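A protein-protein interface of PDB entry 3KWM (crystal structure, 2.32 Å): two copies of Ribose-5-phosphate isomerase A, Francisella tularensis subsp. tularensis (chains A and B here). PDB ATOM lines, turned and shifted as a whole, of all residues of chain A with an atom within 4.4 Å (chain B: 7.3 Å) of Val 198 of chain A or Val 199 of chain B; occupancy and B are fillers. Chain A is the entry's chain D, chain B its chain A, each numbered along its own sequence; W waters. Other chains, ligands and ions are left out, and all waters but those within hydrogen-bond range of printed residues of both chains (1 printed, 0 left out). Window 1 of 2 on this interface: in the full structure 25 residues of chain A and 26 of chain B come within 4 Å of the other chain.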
ATOM      1  N   ILE A 139       4.747  21.502 -10.940  1.00  0.00           N
ATOM      2  CA  ILE A 139       5.788  22.163 -11.698  1.00  0.00           C
ATOM      3  C   ILE A 139       6.496  23.117 -10.738  1.00  0.00           C
ATOM      4  O   ILE A 139       5.861  23.991 -10.144  1.00  0.00           O
ATOM      5  CB  ILE A 139       5.191  22.917 -12.930  1.00  0.00           C
ATOM      6  CG1 ILE A 139       4.455  21.933 -13.849  1.00  0.00           C
ATOM      7  CG2 ILE A 139       6.274  23.663 -13.690  1.00  0.00           C
ATOM      8  CD1 ILE A 139       3.685  22.567 -14.971  1.00  0.00           C
ATOM      9  N   GLU A 140       7.800  22.920 -10.557  1.00  0.00           N
ATOM     10  CA  GLU A 140       8.593  23.847  -9.756  1.00  0.00           C
ATOM     11  C   GLU A 140       9.020  25.026 -10.607  1.00  0.00           C
ATOM     12  O   GLU A 140       9.486  24.870 -11.737  1.00  0.00           O
ATOM     13  CB  GLU A 140       9.809  23.173  -9.118  1.00  0.00           C
ATOM     14  CG  GLU A 140      10.564  24.074  -8.146  1.00  0.00           C
ATOM     15  CD  GLU A 140      11.617  23.323  -7.331  1.00  0.00           C
ATOM     16  OE1 GLU A 140      11.572  22.073  -7.298  1.00  0.00           O
ATOM     17  OE2 GLU A 140      12.487  23.984  -6.725  1.00  0.00           O
ATOM     18  N   ILE A 142      10.485  29.277 -10.666  1.00  0.00           N
ATOM     19  CA  ILE A 142      11.116  30.474 -10.084  1.00  0.00           C
ATOM     20  C   ILE A 142       9.991  31.423  -9.632  1.00  0.00           C
ATOM     21  O   ILE A 142       9.122  31.769 -10.439  1.00  0.00           O
ATOM     22  CB  ILE A 142      12.064  31.192 -11.099  1.00  0.00           C
ATOM     23  CG1 ILE A 142      13.230  30.280 -11.520  1.00  0.00           C
ATOM     24  CG2 ILE A 142      12.574  32.542 -10.548  1.00  0.00           C
ATOM     25  CD1 ILE A 142      14.196  29.917 -10.396  1.00  0.00           C
ATOM     26  N   ILE A 149       4.100  31.949 -15.970  1.00  0.00           N
ATOM     27  CA  ILE A 149       4.057  30.513 -16.266  1.00  0.00           C
ATOM     28  C   ILE A 149       2.637  29.979 -16.184  1.00  0.00           C
ATOM     29  O   ILE A 149       2.218  29.187 -17.038  1.00  0.00           O
ATOM     30  CB  ILE A 149       5.028  29.707 -15.365  1.00  0.00           C
ATOM     31  CG1 ILE A 149       6.482  30.077 -15.702  1.00  0.00           C
ATOM     32  CG2 ILE A 149       4.819  28.206 -15.534  1.00  0.00           C
ATOM     33  CD1 ILE A 149       7.473  29.710 -14.622  1.00  0.00           C
ATOM     34  N   LEU A 192       7.170  21.690 -21.681  1.00  0.00           N
ATOM     35  CA  LEU A 192       7.239  22.383 -20.384  1.00  0.00           C
ATOM     36  C   LEU A 192       8.667  22.794 -19.999  1.00  0.00           C
ATOM     37  O   LEU A 192       8.862  23.812 -19.329  1.00  0.00           O
ATOM     38  CB  LEU A 192       6.606  21.560 -19.263  1.00  0.00           C
ATOM     39  CG  LEU A 192       5.116  21.236 -19.415  1.00  0.00           C
ATOM     40  CD1 LEU A 192       4.711  20.176 -18.408  1.00  0.00           C
ATOM     41  CD2 LEU A 192       4.240  22.485 -19.301  1.00  0.00           C
ATOM     42  N   ILE A 195       9.572  26.360 -21.149  1.00  0.00           N
ATOM     43  CA  ILE A 195       8.943  27.541 -20.553  1.00  0.00           C
ATOM     44  C   ILE A 195       9.910  28.219 -19.586  1.00  0.00           C
ATOM     45  O   ILE A 195      10.371  27.600 -18.616  1.00  0.00           O
ATOM     46  CB  ILE A 195       7.584  27.206 -19.853  1.00  0.00           C
ATOM     47  CG1 ILE A 195       6.593  26.608 -20.861  1.00  0.00           C
ATOM     48  CG2 ILE A 195       6.999  28.458 -19.193  1.00  0.00           C
ATOM     49  CD1 ILE A 195       5.259  26.162 -20.260  1.00  0.00           C
ATOM     50  N   THR A 196      10.223  29.481 -19.866  1.00  0.00           N
ATOM     51  CA  THR A 196      11.133  30.266 -19.035  1.00  0.00           C
ATOM     52  C   THR A 196      10.644  30.406 -17.592  1.00  0.00           C
ATOM     53  O   THR A 196       9.526  30.865 -17.345  1.00  0.00           O
ATOM     54  CB  THR A 196      11.368  31.673 -19.617  1.00  0.00           C
ATOM     55  OG1 THR A 196      11.577  31.580 -21.034  1.00  0.00           O
ATOM     56  CG2 THR A 196      12.580  32.326 -18.953  1.00  0.00           C
ATOM     57  N   GLY A 197      11.507  30.021 -16.652  1.00  0.00           N
ATOM     58  CA  GLY A 197      11.211  30.107 -15.231  1.00  0.00           C
ATOM     59  C   GLY A 197      10.879  28.758 -14.626  1.00  0.00           C
ATOM     60  O   GLY A 197      10.886  28.611 -13.403  1.00  0.00           O
ATOM     61  N   VAL A 198      10.568  27.779 -15.476  1.00  0.00           N
ATOM     62  CA  VAL A 198      10.345  26.413 -15.018  1.00  0.00           C
ATOM     63  C   VAL A 198      11.685  25.814 -14.604  1.00  0.00           C
ATOM     64  O   VAL A 198      12.655  25.846 -15.366  1.00  0.00           O
ATOM     65  CB  VAL A 198       9.618  25.533 -16.087  1.00  0.00           C
ATOM     66  CG1 VAL A 198       9.623  24.058 -15.688  1.00  0.00           C
ATOM     67  CG2 VAL A 198       8.187  26.008 -16.273  1.00  0.00           C
ATOM     68  N   VAL A 199      11.741  25.317 -13.373  1.00  0.00           N
ATOM     69  CA  VAL A 199      12.932  24.673 -12.846  1.00  0.00           C
ATOM     70  C   VAL A 199      12.853  23.194 -13.236  1.00  0.00           C
ATOM     71  O   VAL A 199      13.743  22.677 -13.914  1.00  0.00           O
ATOM     72  CB  VAL A 199      13.052  24.884 -11.307  1.00  0.00           C
ATOM     73  CG1 VAL A 199      14.233  24.119 -10.725  1.00  0.00           C
ATOM     74  CG2 VAL A 199      13.178  26.363 -10.987  1.00  0.00           C
ATOM     75  N   THR A 200      11.749  22.553 -12.853  1.00  0.00           N
ATOM     76  CA  THR A 200      11.477  21.157 -13.144  1.00  0.00           C
ATOM     77  C   THR A 200       9.966  20.992 -13.257  1.00  0.00           C
ATOM     78  O   THR A 200       9.222  21.590 -12.471  1.00  0.00           O
ATOM     79  CB  THR A 200      11.986  20.253 -11.985  1.00  0.00           C
ATOM     80  OG1 THR A 200      13.412  20.363 -11.880  1.00  0.00           O
ATOM     81  CG2 THR A 200      11.649  18.816 -12.208  1.00  0.00           C
ATOM     82  N   ASN A 201       9.517  20.190 -14.226  1.00  0.00           N
ATOM     83  CA  ASN A 201       8.135  19.721 -14.256  1.00  0.00           C
ATOM     84  C   ASN A 201       8.086  18.263 -13.784  1.00  0.00           C
ATOM     85  O   ASN A 201       9.083  17.549 -13.876  1.00  0.00           O
ATOM     86  CB  ASN A 201       7.519  19.894 -15.650  1.00  0.00           C
ATOM     87  CG  ASN A 201       8.067  18.909 -16.666  1.00  0.00           C
ATOM     88  OD1 ASN A 201       7.683  17.747 -16.671  1.00  0.00           O
ATOM     89  ND2 ASN A 201       8.951  19.379 -17.544  1.00  0.00           N
ATOM     90  N   LEU B 106      21.061  36.155 -15.131  1.00  0.00           N
ATOM     91  CA  LEU B 106      20.563  35.360 -16.252  1.00  0.00           C
ATOM     92  C   LEU B 106      19.086  34.943 -16.170  1.00  0.00           C
ATOM     93  O   LEU B 106      18.307  35.178 -17.106  1.00  0.00           O
ATOM     94  CB  LEU B 106      21.447  34.104 -16.391  1.00  0.00           C
ATOM     95  CG  LEU B 106      21.029  33.090 -17.444  1.00  0.00           C
ATOM     96  CD1 LEU B 106      21.016  33.779 -18.776  1.00  0.00           C
ATOM     97  CD2 LEU B 106      21.982  31.916 -17.446  1.00  0.00           C
ATOM     98  N   THR B 107      18.712  34.320 -15.060  1.00  0.00           N
ATOM     99  CA  THR B 107      17.372  33.752 -14.931  1.00  0.00           C
ATOM    100  C   THR B 107      16.269  34.812 -14.928  1.00  0.00           C
ATOM    101  O   THR B 107      15.287  34.686 -15.649  1.00  0.00           O
ATOM    102  CB  THR B 107      17.284  32.806 -13.717  1.00  0.00           C
ATOM    103  OG1 THR B 107      18.183  31.713 -13.929  1.00  0.00           O
ATOM    104  CG2 THR B 107      15.872  32.263 -13.531  1.00  0.00           C
ATOM    105  N   LYS B 110      15.898  36.577 -18.353  1.00  0.00           N
ATOM    106  CA  LYS B 110      15.178  35.759 -19.329  1.00  0.00           C
ATOM    107  C   LYS B 110      13.682  35.706 -19.036  1.00  0.00           C
ATOM    108  O   LYS B 110      12.874  35.667 -19.962  1.00  0.00           O
ATOM    109  CB  LYS B 110      15.770  34.347 -19.437  1.00  0.00           C
ATOM    110  CG  LYS B 110      15.520  33.696 -20.811  1.00  0.00           C
ATOM    111  CD  LYS B 110      16.278  32.379 -20.956  1.00  0.00           C
ATOM    112  CE  LYS B 110      16.324  31.921 -22.400  1.00  0.00           C
ATOM    113  NZ  LYS B 110      17.275  30.785 -22.613  1.00  0.00           N
ATOM    114  N   ILE B 111      13.331  35.695 -17.751  1.00  0.00           N
ATOM    115  CA  ILE B 111      11.940  35.736 -17.319  1.00  0.00           C
ATOM    116  C   ILE B 111      11.303  37.065 -17.728  1.00  0.00           C
ATOM    117  O   ILE B 111      10.175  37.090 -18.231  1.00  0.00           O
ATOM    118  CB  ILE B 111      11.801  35.515 -15.789  1.00  0.00           C
ATOM    119  CG1 ILE B 111      12.052  34.047 -15.433  1.00  0.00           C
ATOM    120  CG2 ILE B 111      10.416  35.956 -15.287  1.00  0.00           C
ATOM    121  CD1 ILE B 111      12.411  33.827 -13.969  1.00  0.00           C
ATOM    122  N   ILE B 139      25.248  29.219 -17.930  1.00  0.00           N
ATOM    123  CA  ILE B 139      24.120  28.340 -17.637  1.00  0.00           C
ATOM    124  C   ILE B 139      23.952  28.329 -16.121  1.00  0.00           C
ATOM    125  O   ILE B 139      24.897  28.013 -15.394  1.00  0.00           O
ATOM    126  CB  ILE B 139      24.355  26.888 -18.153  1.00  0.00           C
ATOM    127  CG1 ILE B 139      24.800  26.893 -19.627  1.00  0.00           C
ATOM    128  CG2 ILE B 139      23.104  26.027 -17.937  1.00  0.00           C
ATOM    129  CD1 ILE B 139      25.056  25.523 -20.224  1.00  0.00           C
ATOM    130  N   GLU B 140      22.769  28.707 -15.649  1.00  0.00           N
ATOM    131  CA  GLU B 140      22.453  28.622 -14.227  1.00  0.00           C
ATOM    132  C   GLU B 140      21.891  27.247 -13.905  1.00  0.00           C
ATOM    133  O   GLU B 140      20.948  26.784 -14.556  1.00  0.00           O
ATOM    134  CB  GLU B 140      21.450  29.704 -13.822  1.00  0.00           C
ATOM    135  CG  GLU B 140      21.215  29.767 -12.317  1.00  0.00           C
ATOM    136  CD  GLU B 140      20.419  30.989 -11.894  1.00  0.00           C
ATOM    137  OE1 GLU B 140      20.407  31.968 -12.668  1.00  0.00           O
ATOM    138  OE2 GLU B 140      19.807  30.970 -10.798  1.00  0.00           O
ATOM    139  N   VAL B 141      22.465  26.598 -12.896  1.00  0.00           N
ATOM    140  CA  VAL B 141      22.097  25.217 -12.586  1.00  0.00           C
ATOM    141  C   VAL B 141      21.832  24.998 -11.092  1.00  0.00           C
ATOM    142  O   VAL B 141      22.379  25.706 -10.239  1.00  0.00           O
ATOM    143  CB  VAL B 141      23.168  24.206 -13.096  1.00  0.00           C
ATOM    144  CG1 VAL B 141      23.482  24.442 -14.576  1.00  0.00           C
ATOM    145  CG2 VAL B 141      24.446  24.287 -12.274  1.00  0.00           C
ATOM    146  N   ILE B 142      20.980  24.021 -10.792  1.00  0.00           N
ATOM    147  CA  ILE B 142      20.773  23.569  -9.421  1.00  0.00           C
ATOM    148  C   ILE B 142      22.097  22.979  -8.927  1.00  0.00           C
ATOM    149  O   ILE B 142      22.625  22.051  -9.547  1.00  0.00           O
ATOM    150  CB  ILE B 142      19.609  22.523  -9.320  1.00  0.00           C
ATOM    151  CG1 ILE B 142      18.291  23.095  -9.886  1.00  0.00           C
ATOM    152  CG2 ILE B 142      19.446  22.002  -7.882  1.00  0.00           C
ATOM    153  CD1 ILE B 142      17.685  24.274  -9.094  1.00  0.00           C
ATOM    154  N   PRO B 143      22.649  23.531  -7.826  1.00  0.00           N
ATOM    155  CA  PRO B 143      23.961  23.139  -7.288  1.00  0.00           C
ATOM    156  C   PRO B 143      24.215  21.632  -7.268  1.00  0.00           C
ATOM    157  O   PRO B 143      25.290  21.188  -7.682  1.00  0.00           O
ATOM    158  CB  PRO B 143      23.934  23.707  -5.862  1.00  0.00           C
ATOM    159  CG  PRO B 143      23.103  24.941  -5.988  1.00  0.00           C
ATOM    160  CD  PRO B 143      22.031  24.605  -7.019  1.00  0.00           C
ATOM    161  N   ILE B 149      25.527  17.882 -15.047  1.00  0.00           N
ATOM    162  CA  ILE B 149      25.327  18.793 -16.167  1.00  0.00           C
ATOM    163  C   ILE B 149      26.614  19.080 -16.957  1.00  0.00           C
ATOM    164  O   ILE B 149      26.587  19.094 -18.198  1.00  0.00           O
ATOM    165  CB  ILE B 149      24.655  20.109 -15.712  1.00  0.00           C
ATOM    166  CG1 ILE B 149      23.264  19.805 -15.146  1.00  0.00           C
ATOM    167  CG2 ILE B 149      24.583  21.113 -16.872  1.00  0.00           C
ATOM    168  CD1 ILE B 149      22.668  20.935 -14.350  1.00  0.00           C
ATOM    169  N   ASN B 170      19.075  33.593  -6.956  1.00  0.00           N
ATOM    170  CA  ASN B 170      18.110  32.501  -6.877  1.00  0.00           C
ATOM    171  C   ASN B 170      18.645  31.316  -6.052  1.00  0.00           C
ATOM    172  O   ASN B 170      17.970  30.292  -5.901  1.00  0.00           O
ATOM    173  CB  ASN B 170      17.711  32.037  -8.284  1.00  0.00           C
ATOM    174  CG  ASN B 170      17.298  33.193  -9.191  1.00  0.00           C
ATOM    175  OD1 ASN B 170      16.360  33.941  -8.886  1.00  0.00           O
ATOM    176  ND2 ASN B 170      17.996  33.340 -10.320  1.00  0.00           N
ATOM    177  N   ASN B 172      21.491  29.644  -6.806  1.00  0.00           N
ATOM    178  CA  ASN B 172      22.037  28.667  -7.742  1.00  0.00           C
ATOM    179  C   ASN B 172      23.486  28.941  -8.142  1.00  0.00           C
ATOM    180  O   ASN B 172      24.053  29.978  -7.799  1.00  0.00           O
ATOM    181  CB  ASN B 172      21.159  28.592  -8.995  1.00  0.00           C
ATOM    182  CG  ASN B 172      19.775  28.051  -8.712  1.00  0.00           C
ATOM    183  OD1 ASN B 172      19.619  27.031  -8.041  1.00  0.00           O
ATOM    184  ND2 ASN B 172      18.761  28.723  -9.239  1.00  0.00           N
ATOM    185  N   VAL B 173      24.083  27.998  -8.863  1.00  0.00           N
ATOM    186  CA  VAL B 173      25.442  28.176  -9.372  1.00  0.00           C
ATOM    187  C   VAL B 173      25.461  28.348 -10.887  1.00  0.00           C
ATOM    188  O   VAL B 173      24.444  28.144 -11.570  1.00  0.00           O
ATOM    189  CB  VAL B 173      26.406  27.041  -8.935  1.00  0.00           C
ATOM    190  CG1 VAL B 173      26.615  27.068  -7.423  1.00  0.00           C
ATOM    191  CG2 VAL B 173      25.910  25.685  -9.391  1.00  0.00           C
ATOM    192  N   LEU B 192      19.699  22.355 -24.270  1.00  0.00           N
ATOM    193  CA  LEU B 192      20.148  22.703 -22.925  1.00  0.00           C
ATOM    194  C   LEU B 192      19.005  22.789 -21.919  1.00  0.00           C
ATOM    195  O   LEU B 192      19.184  22.438 -20.755  1.00  0.00           O
ATOM    196  CB  LEU B 192      20.969  23.995 -22.923  1.00  0.00           C
ATOM    197  CG  LEU B 192      22.259  23.996 -23.747  1.00  0.00           C
ATOM    198  CD1 LEU B 192      22.846  25.387 -23.822  1.00  0.00           C
ATOM    199  CD2 LEU B 192      23.276  23.008 -23.207  1.00  0.00           C
ATOM    200  N   ASN B 193      17.846  23.259 -22.376  1.00  0.00           N
ATOM    201  CA  ASN B 193      16.617  23.281 -21.577  1.00  0.00           C
ATOM    202  C   ASN B 193      16.166  21.888 -21.136  1.00  0.00           C
ATOM    203  O   ASN B 193      15.484  21.750 -20.123  1.00  0.00           O
ATOM    204  CB  ASN B 193      15.469  23.948 -22.354  1.00  0.00           C
ATOM    205  CG  ASN B 193      15.605  25.476 -22.446  1.00  0.00           C
ATOM    206  OD1 ASN B 193      16.482  26.083 -21.826  1.00  0.00           O
ATOM    207  ND2 ASN B 193      14.726  26.098 -23.233  1.00  0.00           N
ATOM    208  N   ILE B 195      18.204  19.389 -20.283  1.00  0.00           N
ATOM    209  CA  ILE B 195      19.121  18.792 -19.306  1.00  0.00           C
ATOM    210  C   ILE B 195      18.594  19.014 -17.880  1.00  0.00           C
ATOM    211  O   ILE B 195      18.415  20.152 -17.446  1.00  0.00           O
ATOM    212  CB  ILE B 195      20.589  19.325 -19.443  1.00  0.00           C
ATOM    213  CG1 ILE B 195      21.143  19.095 -20.856  1.00  0.00           C
ATOM    214  CG2 ILE B 195      21.510  18.666 -18.406  1.00  0.00           C
ATOM    215  CD1 ILE B 195      22.400  19.916 -21.175  1.00  0.00           C
ATOM    216  N   THR B 196      18.343  17.919 -17.167  1.00  0.00           N
ATOM    217  CA  THR B 196      17.834  17.969 -15.794  1.00  0.00           C
ATOM    218  C   THR B 196      18.762  18.749 -14.873  1.00  0.00           C
ATOM    219  O   THR B 196      19.960  18.469 -14.806  1.00  0.00           O
ATOM    220  CB  THR B 196      17.607  16.556 -15.234  1.00  0.00           C
ATOM    221  OG1 THR B 196      16.846  15.805 -16.179  1.00  0.00           O
ATOM    222  CG2 THR B 196      16.834  16.611 -13.923  1.00  0.00           C
ATOM    223  N   GLY B 197      18.197  19.741 -14.186  1.00  0.00           N
ATOM    224  CA  GLY B 197      18.959  20.593 -13.280  1.00  0.00           C
ATOM    225  C   GLY B 197      19.308  21.964 -13.830  1.00  0.00           C
ATOM    226  O   GLY B 197      19.666  22.862 -13.074  1.00  0.00           O
ATOM    227  N   VAL B 198      19.233  22.121 -15.148  1.00  0.00           N
ATOM    228  CA  VAL B 198      19.405  23.430 -15.784  1.00  0.00           C
ATOM    229  C   VAL B 198      18.198  24.299 -15.444  1.00  0.00           C
ATOM    230  O   VAL B 198      17.056  23.887 -15.648  1.00  0.00           O
ATOM    231  CB  VAL B 198      19.575  23.313 -17.328  1.00  0.00           C
ATOM    232  CG1 VAL B 198      19.416  24.675 -18.010  1.00  0.00           C
ATOM    233  CG2 VAL B 198      20.920  22.692 -17.671  1.00  0.00           C
ATOM    234  N   VAL B 199      18.456  25.483 -14.896  1.00  0.00           N
ATOM    235  CA  VAL B 199      17.400  26.437 -14.601  1.00  0.00           C
ATOM    236  C   VAL B 199      17.161  27.281 -15.858  1.00  0.00           C
ATOM    237  O   VAL B 199      16.051  27.354 -16.368  1.00  0.00           O
ATOM    238  CB  VAL B 199      17.750  27.329 -13.373  1.00  0.00           C
ATOM    239  CG1 VAL B 199      16.648  28.353 -13.096  1.00  0.00           C
ATOM    240  CG2 VAL B 199      18.001  26.473 -12.135  1.00  0.00           C
ATOM    241  N   THR B 200      18.230  27.890 -16.357  1.00  0.00           N
ATOM    242  CA  THR B 200      18.182  28.777 -17.503  1.00  0.00           C
ATOM    243  C   THR B 200      19.531  28.682 -18.209  1.00  0.00           C
ATOM    244  O   THR B 200      20.561  28.520 -17.559  1.00  0.00           O
ATOM    245  CB  THR B 200      17.913  30.230 -17.038  1.00  0.00           C
ATOM    246  OG1 THR B 200      16.610  30.299 -16.453  1.00  0.00           O
ATOM    247  CG2 THR B 200      17.943  31.197 -18.183  1.00  0.00           C
ATOM    248  N   ASN B 201      19.518  28.755 -19.536  1.00  0.00           N
ATOM    249  CA  ASN B 201      20.744  28.969 -20.295  1.00  0.00           C
ATOM    250  C   ASN B 201      20.760  30.358 -20.951  1.00  0.00           C
ATOM    251  O   ASN B 201      19.704  30.941 -21.204  1.00  0.00           O
ATOM    252  CB  ASN B 201      20.970  27.845 -21.308  1.00  0.00           C
ATOM    253  CG  ASN B 201      20.030  27.922 -22.488  1.00  0.00           C
ATOM    254  OD1 ASN B 201      20.258  28.693 -23.417  1.00  0.00           O
ATOM    255  ND2 ASN B 201      18.974  27.108 -22.470  1.00  0.00           N
HETATM  256  O   HOH W   1      15.829  21.138 -14.765  1.00  0.00           O
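Of chain A, only Ile 142 (3.97 Å) and Val 198 (3.8 Å) come within 4 Å of Val 199 of chain B. Of the printed residues of chain A, Ile 142 of chain B touches Val 199. Printed residues of chain A within 4 Å of Thr 107 of chain B: Ile 142 (3.9 Å). Of the printed residues of chain B, Thr 196 of chain A touches Lys 110 (3.5 Å) and Ile 111 (3.7 Å). Printed residues of chain A within 4 Å of Ile 111 of chain B: Ile 142 (3.7 Å) and Thr 196 (3.7 Å). Printed residues of chain B within 4 Å of Ile 142 of chain A: Thr 107, Ile 111 and Val 199. Ile 195 of chain A touches none of the printed residues of chain B. The nearest printed residue of chain A that does not touch Lys 110 of chain B is Gly 197 of chain A (6.5 Å).
Water W1 lies within hydrogen-bond range of O of Val 199 of chain A, N of Gly 197 of chain B and O of Val 198 of chain B.
Among the printed residues, pairs that only touch across the chains: Thr 196 of chain A with Lys 110 of chain B, Thr 196 of chain A with Ile 111 of chain B, Ile 142 of chain A with Ile 111 of chain B, Val 199 of chain A with Ile 142 of chain B, Val 198 of chain A with Val 199 of chain B, Ile 142 of chain A with Thr 107 of chain B, Val 199 of chain A with Val 198 of chain B and Ile 142 of chain A with Val 199 of chain B.
Ile 142 of chain A touches Val 199 of chain B, and with the chains exchanged Val 199 of chain A touches Ile 142 of chain B. Val 198 of chain A touches Val 199 of chain B, and with the chains exchanged Val 199 of chain A touches Val 198 of chain B. Of the 8 pairs that touch across the chains among the printed residues, 4 have their exchanged pair printed and touching as well.
Hydrophobic or aromatic side chains of chain B within 4 Å of the printed part of chain A: Ile 111, Ile 142 and Val 199. Of the 12 printed residues of chain A, 4 touch a printed residue of chain B. Hydrophobic or aromatic side chains of chain A that line the printed part of chain B: Ile 142 and Val 199. Among the printed residues, 8 pairs touch across the chains.
The backbone NH of Ile 142 of chain B is in hydrogen-bond range of the backbone carbonyl oxygen of Gly 197 of chain B, 2.9 Å away. The side-chain hydroxyl of Thr 200 of chain B sits at hydrogen-bond distance from the side-chain hydroxyl of Thr 107 of chain B (3.3 Å). The backbone carbonyl oxygen (O) of Glu 140 of chain B lies within hydrogen-bond range of the backbone NH (N) of Val 199 of chain B (2.8 Å). N of Ile 142 of chain A is in hydrogen-bond range of O of Gly 197 of chain A. NZ of Lys 110 of chain B sits at hydrogen-bond distance from O of Asn 201 of chain B (2.8 Å). O of Glu 140 of chain A lies within hydrogen-bond range of N of Val 199 of chain A (2.8 Å).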
